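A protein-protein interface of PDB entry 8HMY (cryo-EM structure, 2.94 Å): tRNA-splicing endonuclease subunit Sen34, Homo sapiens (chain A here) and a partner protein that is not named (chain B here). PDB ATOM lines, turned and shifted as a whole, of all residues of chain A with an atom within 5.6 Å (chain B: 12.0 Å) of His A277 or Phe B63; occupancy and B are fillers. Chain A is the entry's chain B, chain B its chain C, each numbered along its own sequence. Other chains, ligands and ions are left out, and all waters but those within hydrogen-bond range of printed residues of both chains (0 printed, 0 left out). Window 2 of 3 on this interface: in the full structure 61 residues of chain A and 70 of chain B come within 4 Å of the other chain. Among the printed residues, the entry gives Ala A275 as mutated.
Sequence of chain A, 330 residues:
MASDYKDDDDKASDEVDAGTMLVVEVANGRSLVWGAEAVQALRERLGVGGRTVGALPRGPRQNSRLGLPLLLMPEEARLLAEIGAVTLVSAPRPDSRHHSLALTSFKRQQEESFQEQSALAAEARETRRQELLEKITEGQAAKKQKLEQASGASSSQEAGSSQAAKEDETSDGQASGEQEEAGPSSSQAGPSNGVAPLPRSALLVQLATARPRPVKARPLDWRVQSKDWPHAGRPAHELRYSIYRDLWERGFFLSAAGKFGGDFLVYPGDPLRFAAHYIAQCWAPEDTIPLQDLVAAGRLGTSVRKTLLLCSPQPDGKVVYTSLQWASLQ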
ATOM      1  N   VAL A 266     -11.961  26.452 -30.652  1.00  0.00           N
ATOM      2  CA  VAL A 266     -11.975  25.005 -30.484  1.00  0.00           C
ATOM      3  C   VAL A 266     -12.601  24.677 -29.137  1.00  0.00           C
ATOM      4  O   VAL A 266     -12.098  25.099 -28.091  1.00  0.00           O
ATOM      5  CB  VAL A 266     -10.563  24.414 -30.594  1.00  0.00           C
ATOM      6  CG1 VAL A 266     -10.638  22.963 -30.966  1.00  0.00           C
ATOM      7  CG2 VAL A 266      -9.746  25.178 -31.618  1.00  0.00           C
ATOM      8  N   TYR A 267     -13.682  23.921 -29.157  1.00  0.00           N
ATOM      9  CA  TYR A 267     -14.427  23.598 -27.954  1.00  0.00           C
ATOM     10  C   TYR A 267     -14.186  22.156 -27.535  1.00  0.00           C
ATOM     11  O   TYR A 267     -14.152  21.262 -28.384  1.00  0.00           O
ATOM     12  CB  TYR A 267     -15.932  23.796 -28.158  1.00  0.00           C
ATOM     13  CG  TYR A 267     -16.341  25.202 -28.490  1.00  0.00           C
ATOM     14  CD1 TYR A 267     -16.584  26.125 -27.493  1.00  0.00           C
ATOM     15  CD2 TYR A 267     -16.493  25.605 -29.801  1.00  0.00           C
ATOM     16  CE1 TYR A 267     -16.954  27.408 -27.791  1.00  0.00           C
ATOM     17  CE2 TYR A 267     -16.864  26.885 -30.109  1.00  0.00           C
ATOM     18  CZ  TYR A 267     -17.094  27.782 -29.101  1.00  0.00           C
ATOM     19  OH  TYR A 267     -17.465  29.064 -29.407  1.00  0.00           O
ATOM     20  N   PRO A 268     -14.032  21.895 -26.238  1.00  0.00           N
ATOM     21  CA  PRO A 268     -14.010  20.500 -25.774  1.00  0.00           C
ATOM     22  C   PRO A 268     -15.301  19.755 -26.046  1.00  0.00           C
ATOM     23  O   PRO A 268     -15.273  18.526 -26.165  1.00  0.00           O
ATOM     24  CB  PRO A 268     -13.751  20.641 -24.269  1.00  0.00           C
ATOM     25  CG  PRO A 268     -14.153  22.038 -23.940  1.00  0.00           C
ATOM     26  CD  PRO A 268     -13.810  22.844 -25.138  1.00  0.00           C
ATOM     27  N   PHE A 274     -20.179  24.213 -23.078  1.00  0.00           N
ATOM     28  CA  PHE A 274     -18.744  24.293 -22.854  1.00  0.00           C
ATOM     29  C   PHE A 274     -18.170  25.571 -23.446  1.00  0.00           C
ATOM     30  O   PHE A 274     -18.736  26.177 -24.357  1.00  0.00           O
ATOM     31  CB  PHE A 274     -18.034  23.077 -23.443  1.00  0.00           C
ATOM     32  CG  PHE A 274     -18.394  21.797 -22.767  1.00  0.00           C
ATOM     33  CD1 PHE A 274     -17.733  21.396 -21.631  1.00  0.00           C
ATOM     34  CD2 PHE A 274     -19.413  21.002 -23.256  1.00  0.00           C
ATOM     35  CE1 PHE A 274     -18.071  20.229 -21.002  1.00  0.00           C
ATOM     36  CE2 PHE A 274     -19.751  19.829 -22.632  1.00  0.00           C
ATOM     37  CZ  PHE A 274     -19.078  19.442 -21.504  1.00  0.00           C
ATOM     38  N   ALA A 275     -17.029  25.975 -22.907  1.00  0.00           N
ATOM     39  CA  ALA A 275     -16.317  27.156 -23.352  1.00  0.00           C
ATOM     40  C   ALA A 275     -15.055  26.746 -24.096  1.00  0.00           C
ATOM     41  O   ALA A 275     -14.421  25.741 -23.770  1.00  0.00           O
ATOM     42  CB  ALA A 275     -15.958  28.057 -22.171  1.00  0.00           C
ATOM     43  N   ALA A 276     -14.703  27.532 -25.108  1.00  0.00           N
ATOM     44  CA  ALA A 276     -13.544  27.221 -25.928  1.00  0.00           C
ATOM     45  C   ALA A 276     -12.271  27.230 -25.094  1.00  0.00           C
ATOM     46  O   ALA A 276     -12.131  28.017 -24.156  1.00  0.00           O
ATOM     47  CB  ALA A 276     -13.428  28.226 -27.067  1.00  0.00           C
ATOM     48  N   HIS A 277     -11.343  26.339 -25.431  1.00  0.00           N
ATOM     49  CA  HIS A 277     -10.047  26.303 -24.769  1.00  0.00           C
ATOM     50  C   HIS A 277      -8.946  26.956 -25.581  1.00  0.00           C
ATOM     51  O   HIS A 277      -8.030  27.536 -24.995  1.00  0.00           O
ATOM     52  CB  HIS A 277      -9.633  24.863 -24.463  1.00  0.00           C
ATOM     53  CG  HIS A 277     -10.404  24.229 -23.348  1.00  0.00           C
ATOM     54  ND1 HIS A 277     -10.462  22.865 -23.170  1.00  0.00           N
ATOM     55  CD2 HIS A 277     -11.148  24.770 -22.356  1.00  0.00           C
ATOM     56  CE1 HIS A 277     -11.210  22.592 -22.117  1.00  0.00           C
ATOM     57  NE2 HIS A 277     -11.639  23.730 -21.605  1.00  0.00           N
ATOM     58  N   TYR A 278      -9.000  26.880 -26.906  1.00  0.00           N
ATOM     59  CA  TYR A 278      -7.928  27.388 -27.746  1.00  0.00           C
ATOM     60  C   TYR A 278      -8.482  28.351 -28.781  1.00  0.00           C
ATOM     61  O   TYR A 278      -9.668  28.319 -29.112  1.00  0.00           O
ATOM     62  CB  TYR A 278      -7.172  26.262 -28.466  1.00  0.00           C
ATOM     63  CG  TYR A 278      -6.971  25.007 -27.653  1.00  0.00           C
ATOM     64  CD1 TYR A 278      -5.830  24.825 -26.890  1.00  0.00           C
ATOM     65  CD2 TYR A 278      -7.919  23.995 -27.666  1.00  0.00           C
ATOM     66  CE1 TYR A 278      -5.647  23.680 -26.150  1.00  0.00           C
ATOM     67  CE2 TYR A 278      -7.744  22.850 -26.932  1.00  0.00           C
ATOM     68  CZ  TYR A 278      -6.609  22.694 -26.178  1.00  0.00           C
ATOM     69  OH  TYR A 278      -6.445  21.542 -25.448  1.00  0.00           O
ATOM     70  N   ILE A 279      -7.611  29.226 -29.268  1.00  0.00           N
ATOM     71  CA  ILE A 279      -7.862  30.013 -30.466  1.00  0.00           C
ATOM     72  C   ILE A 279      -6.931  29.487 -31.548  1.00  0.00           C
ATOM     73  O   ILE A 279      -5.709  29.473 -31.370  1.00  0.00           O
ATOM     74  CB  ILE A 279      -7.635  31.512 -30.224  1.00  0.00           C
ATOM     75  CG1 ILE A 279      -8.458  32.004 -29.037  1.00  0.00           C
ATOM     76  CG2 ILE A 279      -8.002  32.305 -31.455  1.00  0.00           C
ATOM     77  CD1 ILE A 279      -8.013  33.355 -28.516  1.00  0.00           C
ATOM     78  N   ARG A 305      -8.663  33.782 -21.179  1.00  0.00           N
ATOM     79  CA  ARG A 305      -8.404  32.436 -20.657  1.00  0.00           C
ATOM     80  C   ARG A 305      -8.561  31.363 -21.737  1.00  0.00           C
ATOM     81  O   ARG A 305      -9.308  30.398 -21.577  1.00  0.00           O
ATOM     82  CB  ARG A 305      -9.292  32.127 -19.451  1.00  0.00           C
ATOM     83  CG  ARG A 305      -9.053  33.023 -18.255  1.00  0.00           C
ATOM     84  CD  ARG A 305     -10.052  32.703 -17.170  1.00  0.00           C
ATOM     85  NE  ARG A 305     -10.260  31.265 -17.070  1.00  0.00           N
ATOM     86  CZ  ARG A 305      -9.697  30.496 -16.147  1.00  0.00           C
ATOM     87  NH1 ARG A 305      -8.898  31.033 -15.236  1.00  0.00           N
ATOM     88  NH2 ARG A 305      -9.935  29.193 -16.134  1.00  0.00           N
ATOM     89  N   LYS A 306      -7.848  31.546 -22.846  1.00  0.00           N
ATOM     90  CA  LYS A 306      -7.766  30.557 -23.909  1.00  0.00           C
ATOM     91  C   LYS A 306      -6.325  30.461 -24.379  1.00  0.00           C
ATOM     92  O   LYS A 306      -5.636  31.479 -24.488  1.00  0.00           O
ATOM     93  CB  LYS A 306      -8.653  30.913 -25.103  1.00  0.00           C
ATOM     94  CG  LYS A 306     -10.078  31.237 -24.766  1.00  0.00           C
ATOM     95  CD  LYS A 306     -10.897  31.322 -26.022  1.00  0.00           C
ATOM     96  CE  LYS A 306     -12.340  31.597 -25.709  1.00  0.00           C
ATOM     97  NZ  LYS A 306     -12.746  30.979 -24.432  1.00  0.00           N
ATOM     98  N   THR A 307      -5.874  29.244 -24.657  1.00  0.00           N
ATOM     99  CA  THR A 307      -4.550  29.057 -25.229  1.00  0.00           C
ATOM    100  C   THR A 307      -4.562  29.444 -26.703  1.00  0.00           C
ATOM    101  O   THR A 307      -5.565  29.287 -27.397  1.00  0.00           O
ATOM    102  CB  THR A 307      -4.106  27.603 -25.058  1.00  0.00           C
ATOM    103  OG1 THR A 307      -4.090  27.275 -23.667  1.00  0.00           O
ATOM    104  CG2 THR A 307      -2.720  27.386 -25.610  1.00  0.00           C
ATOM    105  N   SER B  57     -27.823  29.595 -22.153  1.00  0.00           N
ATOM    106  CA  SER B  57     -27.178  28.543 -21.381  1.00  0.00           C
ATOM    107  C   SER B  57     -27.719  28.616 -19.965  1.00  0.00           C
ATOM    108  O   SER B  57     -27.596  29.652 -19.303  1.00  0.00           O
ATOM    109  CB  SER B  57     -25.655  28.690 -21.397  1.00  0.00           C
ATOM    110  OG  SER B  57     -25.265  30.052 -21.393  1.00  0.00           O
ATOM    111  N   GLY B  59     -27.313  28.688 -16.921  1.00  0.00           N
ATOM    112  CA  GLY B  59     -26.263  28.860 -15.947  1.00  0.00           C
ATOM    113  C   GLY B  59     -24.932  29.187 -16.590  1.00  0.00           C
ATOM    114  O   GLY B  59     -24.854  29.544 -17.768  1.00  0.00           O
ATOM    115  N   PRO B  60     -23.854  29.079 -15.822  1.00  0.00           N
ATOM    116  CA  PRO B  60     -22.518  29.316 -16.373  1.00  0.00           C
ATOM    117  C   PRO B  60     -22.029  28.121 -17.185  1.00  0.00           C
ATOM    118  O   PRO B  60     -22.620  27.042 -17.183  1.00  0.00           O
ATOM    119  CB  PRO B  60     -21.648  29.534 -15.125  1.00  0.00           C
ATOM    120  CG  PRO B  60     -22.615  29.739 -13.996  1.00  0.00           C
ATOM    121  CD  PRO B  60     -23.819  28.939 -14.360  1.00  0.00           C
ATOM    122  N   LYS B  61     -20.918  28.339 -17.881  1.00  0.00           N
ATOM    123  CA  LYS B  61     -20.356  27.348 -18.785  1.00  0.00           C
ATOM    124  C   LYS B  61     -19.336  26.469 -18.073  1.00  0.00           C
ATOM    125  O   LYS B  61     -18.715  26.875 -17.088  1.00  0.00           O
ATOM    126  CB  LYS B  61     -19.703  28.030 -19.986  1.00  0.00           C
ATOM    127  CG  LYS B  61     -20.685  28.569 -21.007  1.00  0.00           C
ATOM    128  CD  LYS B  61     -20.063  29.705 -21.790  1.00  0.00           C
ATOM    129  CE  LYS B  61     -20.856  30.021 -23.034  1.00  0.00           C
ATOM    130  NZ  LYS B  61     -20.250  31.152 -23.781  1.00  0.00           N
ATOM    131  N   ASP B  62     -19.164  25.256 -18.593  1.00  0.00           N
ATOM    132  CA  ASP B  62     -18.293  24.260 -17.994  1.00  0.00           C
ATOM    133  C   ASP B  62     -16.883  24.386 -18.562  1.00  0.00           C
ATOM    134  O   ASP B  62     -16.623  25.174 -19.474  1.00  0.00           O
ATOM    135  CB  ASP B  62     -18.861  22.864 -18.233  1.00  0.00           C
ATOM    136  CG  ASP B  62     -20.349  22.793 -17.962  1.00  0.00           C
ATOM    137  OD1 ASP B  62     -20.958  23.859 -17.743  1.00  0.00           O
ATOM    138  OD2 ASP B  62     -20.913  21.680 -17.982  1.00  0.00           O
ATOM    139  N   PHE B  63     -15.951  23.608 -18.011  1.00  0.00           N
ATOM    140  CA  PHE B  63     -14.564  23.637 -18.465  1.00  0.00           C
ATOM    141  C   PHE B  63     -14.123  22.306 -19.059  1.00  0.00           C
ATOM    142  O   PHE B  63     -13.683  22.274 -20.212  1.00  0.00           O
ATOM    143  CB  PHE B  63     -13.637  24.046 -17.312  1.00  0.00           C
ATOM    144  CG  PHE B  63     -12.195  24.187 -17.714  1.00  0.00           C
ATOM    145  CD1 PHE B  63     -11.306  23.142 -17.539  1.00  0.00           C
ATOM    146  CD2 PHE B  63     -11.731  25.366 -18.267  1.00  0.00           C
ATOM    147  CE1 PHE B  63      -9.984  23.269 -17.910  1.00  0.00           C
ATOM    148  CE2 PHE B  63     -10.407  25.497 -18.638  1.00  0.00           C
ATOM    149  CZ  PHE B  63      -9.535  24.447 -18.459  1.00  0.00           C
ATOM    150  N   LEU B  64     -14.227  21.208 -18.318  1.00  0.00           N
ATOM    151  CA  LEU B  64     -13.763  19.947 -18.871  1.00  0.00           C
ATOM    152  C   LEU B  64     -14.940  19.037 -19.198  1.00  0.00           C
ATOM    153  O   LEU B  64     -15.945  19.041 -18.481  1.00  0.00           O
ATOM    154  CB  LEU B  64     -12.816  19.230 -17.902  1.00  0.00           C
ATOM    155  CG  LEU B  64     -11.346  19.665 -17.954  1.00  0.00           C
ATOM    156  CD1 LEU B  64     -10.518  18.894 -16.940  1.00  0.00           C
ATOM    157  CD2 LEU B  64     -10.768  19.501 -19.351  1.00  0.00           C
ATOM    158  N   PRO B  65     -14.842  18.246 -20.265  1.00  0.00           N
ATOM    159  CA  PRO B  65     -16.009  17.495 -20.738  1.00  0.00           C
ATOM    160  C   PRO B  65     -16.190  16.152 -20.056  1.00  0.00           C
ATOM    161  O   PRO B  65     -16.928  15.301 -20.560  1.00  0.00           O
ATOM    162  CB  PRO B  65     -15.727  17.317 -22.235  1.00  0.00           C
ATOM    163  CG  PRO B  65     -14.269  17.707 -22.435  1.00  0.00           C
ATOM    164  CD  PRO B  65     -13.664  17.981 -21.099  1.00  0.00           C
ATOM    165  N   ASP B  66     -15.519  15.933 -18.930  1.00  0.00           N
ATOM    166  CA  ASP B  66     -15.631  14.680 -18.194  1.00  0.00           C
ATOM    167  C   ASP B  66     -16.701  14.834 -17.120  1.00  0.00           C
ATOM    168  O   ASP B  66     -16.504  15.545 -16.129  1.00  0.00           O
ATOM    169  CB  ASP B  66     -14.290  14.276 -17.587  1.00  0.00           C
ATOM    170  CG  ASP B  66     -14.000  12.799 -17.767  1.00  0.00           C
ATOM    171  OD1 ASP B  66     -14.769  12.126 -18.482  1.00  0.00           O
ATOM    172  OD2 ASP B  66     -13.002  12.313 -17.194  1.00  0.00           O
ATOM    173  N   GLY B  67     -17.832  14.164 -17.323  1.00  0.00           N
ATOM    174  CA  GLY B  67     -18.925  14.175 -16.372  1.00  0.00           C
ATOM    175  C   GLY B  67     -19.738  12.910 -16.537  1.00  0.00           C
ATOM    176  O   GLY B  67     -19.510  12.113 -17.452  1.00  0.00           O
ATOM    177  N   ALA B  70     -24.669  15.258 -14.958  1.00  0.00           N
ATOM    178  CA  ALA B  70     -24.957  16.688 -14.972  1.00  0.00           C
ATOM    179  C   ALA B  70     -24.688  17.284 -16.348  1.00  0.00           C
ATOM    180  O   ALA B  70     -25.534  17.993 -16.907  1.00  0.00           O
ATOM    181  CB  ALA B  70     -24.130  17.397 -13.901  1.00  0.00           C
ATOM    182  N   GLN B  71     -23.508  17.001 -16.907  1.00  0.00           N
ATOM    183  CA  GLN B  71     -23.159  17.509 -18.229  1.00  0.00           C
ATOM    184  C   GLN B  71     -24.159  17.040 -19.278  1.00  0.00           C
ATOM    185  O   GLN B  71     -24.670  17.841 -20.071  1.00  0.00           O
ATOM    186  CB  GLN B  71     -21.747  17.058 -18.602  1.00  0.00           C
ATOM    187  CG  GLN B  71     -20.721  17.177 -17.486  1.00  0.00           C
ATOM    188  CD  GLN B  71     -20.053  18.531 -17.443  1.00  0.00           C
ATOM    189  OE1 GLN B  71     -18.844  18.644 -17.636  1.00  0.00           O
ATOM    190  NE2 GLN B  71     -20.835  19.568 -17.178  1.00  0.00           N
ATOM    191  N   ALA B  72     -24.458  15.738 -19.285  1.00  0.00           N
ATOM    192  CA  ALA B  72     -25.360  15.185 -20.288  1.00  0.00           C
ATOM    193  C   ALA B  72     -26.765  15.753 -20.152  1.00  0.00           C
ATOM    194  O   ALA B  72     -27.395  16.099 -21.156  1.00  0.00           O
ATOM    195  CB  ALA B  72     -25.388  13.661 -20.184  1.00  0.00           C
ATOM    196  N   ARG B  74     -27.774  18.659 -18.710  1.00  0.00           N
ATOM    197  CA  ARG B  74     -27.847  20.068 -19.065  1.00  0.00           C
ATOM    198  C   ARG B  74     -27.676  20.277 -20.563  1.00  0.00           C
ATOM    199  O   ARG B  74     -28.327  21.158 -21.141  1.00  0.00           O
ATOM    200  CB  ARG B  74     -26.814  20.864 -18.274  1.00  0.00           C
ATOM    201  CG  ARG B  74     -27.295  21.244 -16.885  1.00  0.00           C
ATOM    202  CD  ARG B  74     -26.376  22.249 -16.219  1.00  0.00           C
ATOM    203  NE  ARG B  74     -25.015  21.741 -16.096  1.00  0.00           N
ATOM    204  CZ  ARG B  74     -24.635  20.834 -15.204  1.00  0.00           C
ATOM    205  NH1 ARG B  74     -25.515  20.333 -14.349  1.00  0.00           N
ATOM    206  NH2 ARG B  74     -23.374  20.430 -15.164  1.00  0.00           N
ATOM    207  N   LEU B  75     -26.850  19.460 -21.220  1.00  0.00           N
ATOM    208  CA  LEU B  75     -26.722  19.573 -22.668  1.00  0.00           C
ATOM    209  C   LEU B  75     -28.006  19.151 -23.369  1.00  0.00           C
ATOM    210  O   LEU B  75     -28.444  19.808 -24.320  1.00  0.00           O
ATOM    211  CB  LEU B  75     -25.547  18.735 -23.158  1.00  0.00           C
ATOM    212  CG  LEU B  75     -25.179  18.926 -24.623  1.00  0.00           C
ATOM    213  CD1 LEU B  75     -24.745  20.353 -24.861  1.00  0.00           C
ATOM    214  CD2 LEU B  75     -24.083  17.965 -25.006  1.00  0.00           C
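Among the printed residues, no Asp or Glu carboxylate lies within 4 Å of a Lys or Arg side-chain nitrogen of the other chain.
His A277 touches just one residue of chain B: Phe B63.
Phe B63 touches just these residues of chain A: Pro A268 (3.8 Å) and His A277 (2.9 Å).
No residue of chain B comes within 4 Å of Val A266.
No residue of chain B comes within 4 Å of Tyr A267.
Phe A274 touches four residues of chain B.
Of chain B, only Asp B62 (3.5 Å) comes within 4 Å of Ala A275.
No residue of chain B comes within 4 Å of Ala A276.
No residue of chain B comes within 4 Å of Tyr A278.
No residue of chain B comes within 4 Å of Arg A305.
No residue of chain B comes within 4 Å of Lys A306.
No residue of chain B comes within 4 Å of Thr A307.
Of the printed residues of chain A, Leu B64 touches Phe A274.
Of the printed residues of chain A, Gln B71 touches Phe A274.
Of the printed residues of chain A, Pro B65 touches Pro A268 and Phe A274.
Printed residues of chain A within 4 Å of Asp B62: Phe A274 and Ala A275.
The nearest residue of chain B that does not touch His A277 is Leu B64 (4.2 Å).
CG of Pro A268 touches O of Phe B63 (3.8 Å).
CB of Pro A268 touches CG of Pro B65, 3.5 Å away.
Phe A274 touches Asp B62 (CD1 to CB, 3.9 Å).
CE1 of Phe A274 touches O of Leu B64, at 3.5 Å.
Pro B65 touches Phe A274 (CA to CE1, 3.4 Å).
Phe A274 touches Gln B71 (CE1 to OE1, 3.8 Å).
N of Ala A275 touches O of Asp B62 (3.5 Å).
The backbone NH (N) of His A277 is in hydrogen-bond range of the backbone carbonyl oxygen (O) of Val A266.
N of Thr A307 lies within hydrogen-bond range of O of His A277 (2.8 Å).
The side-chain carboxylate of Asp B62 is in salt-bridge range of the guanidinium group of Arg B74.
OE1 of Gln B71 sits close to O of Leu B64, at 3.0 Å.
NE2 of Gln B71 lies close to NH2 of Arg B74, at 3.4 Å.
NE2 of His A277 lies within hydrogen-bond range of O of Phe B63, 2.9 Å away.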
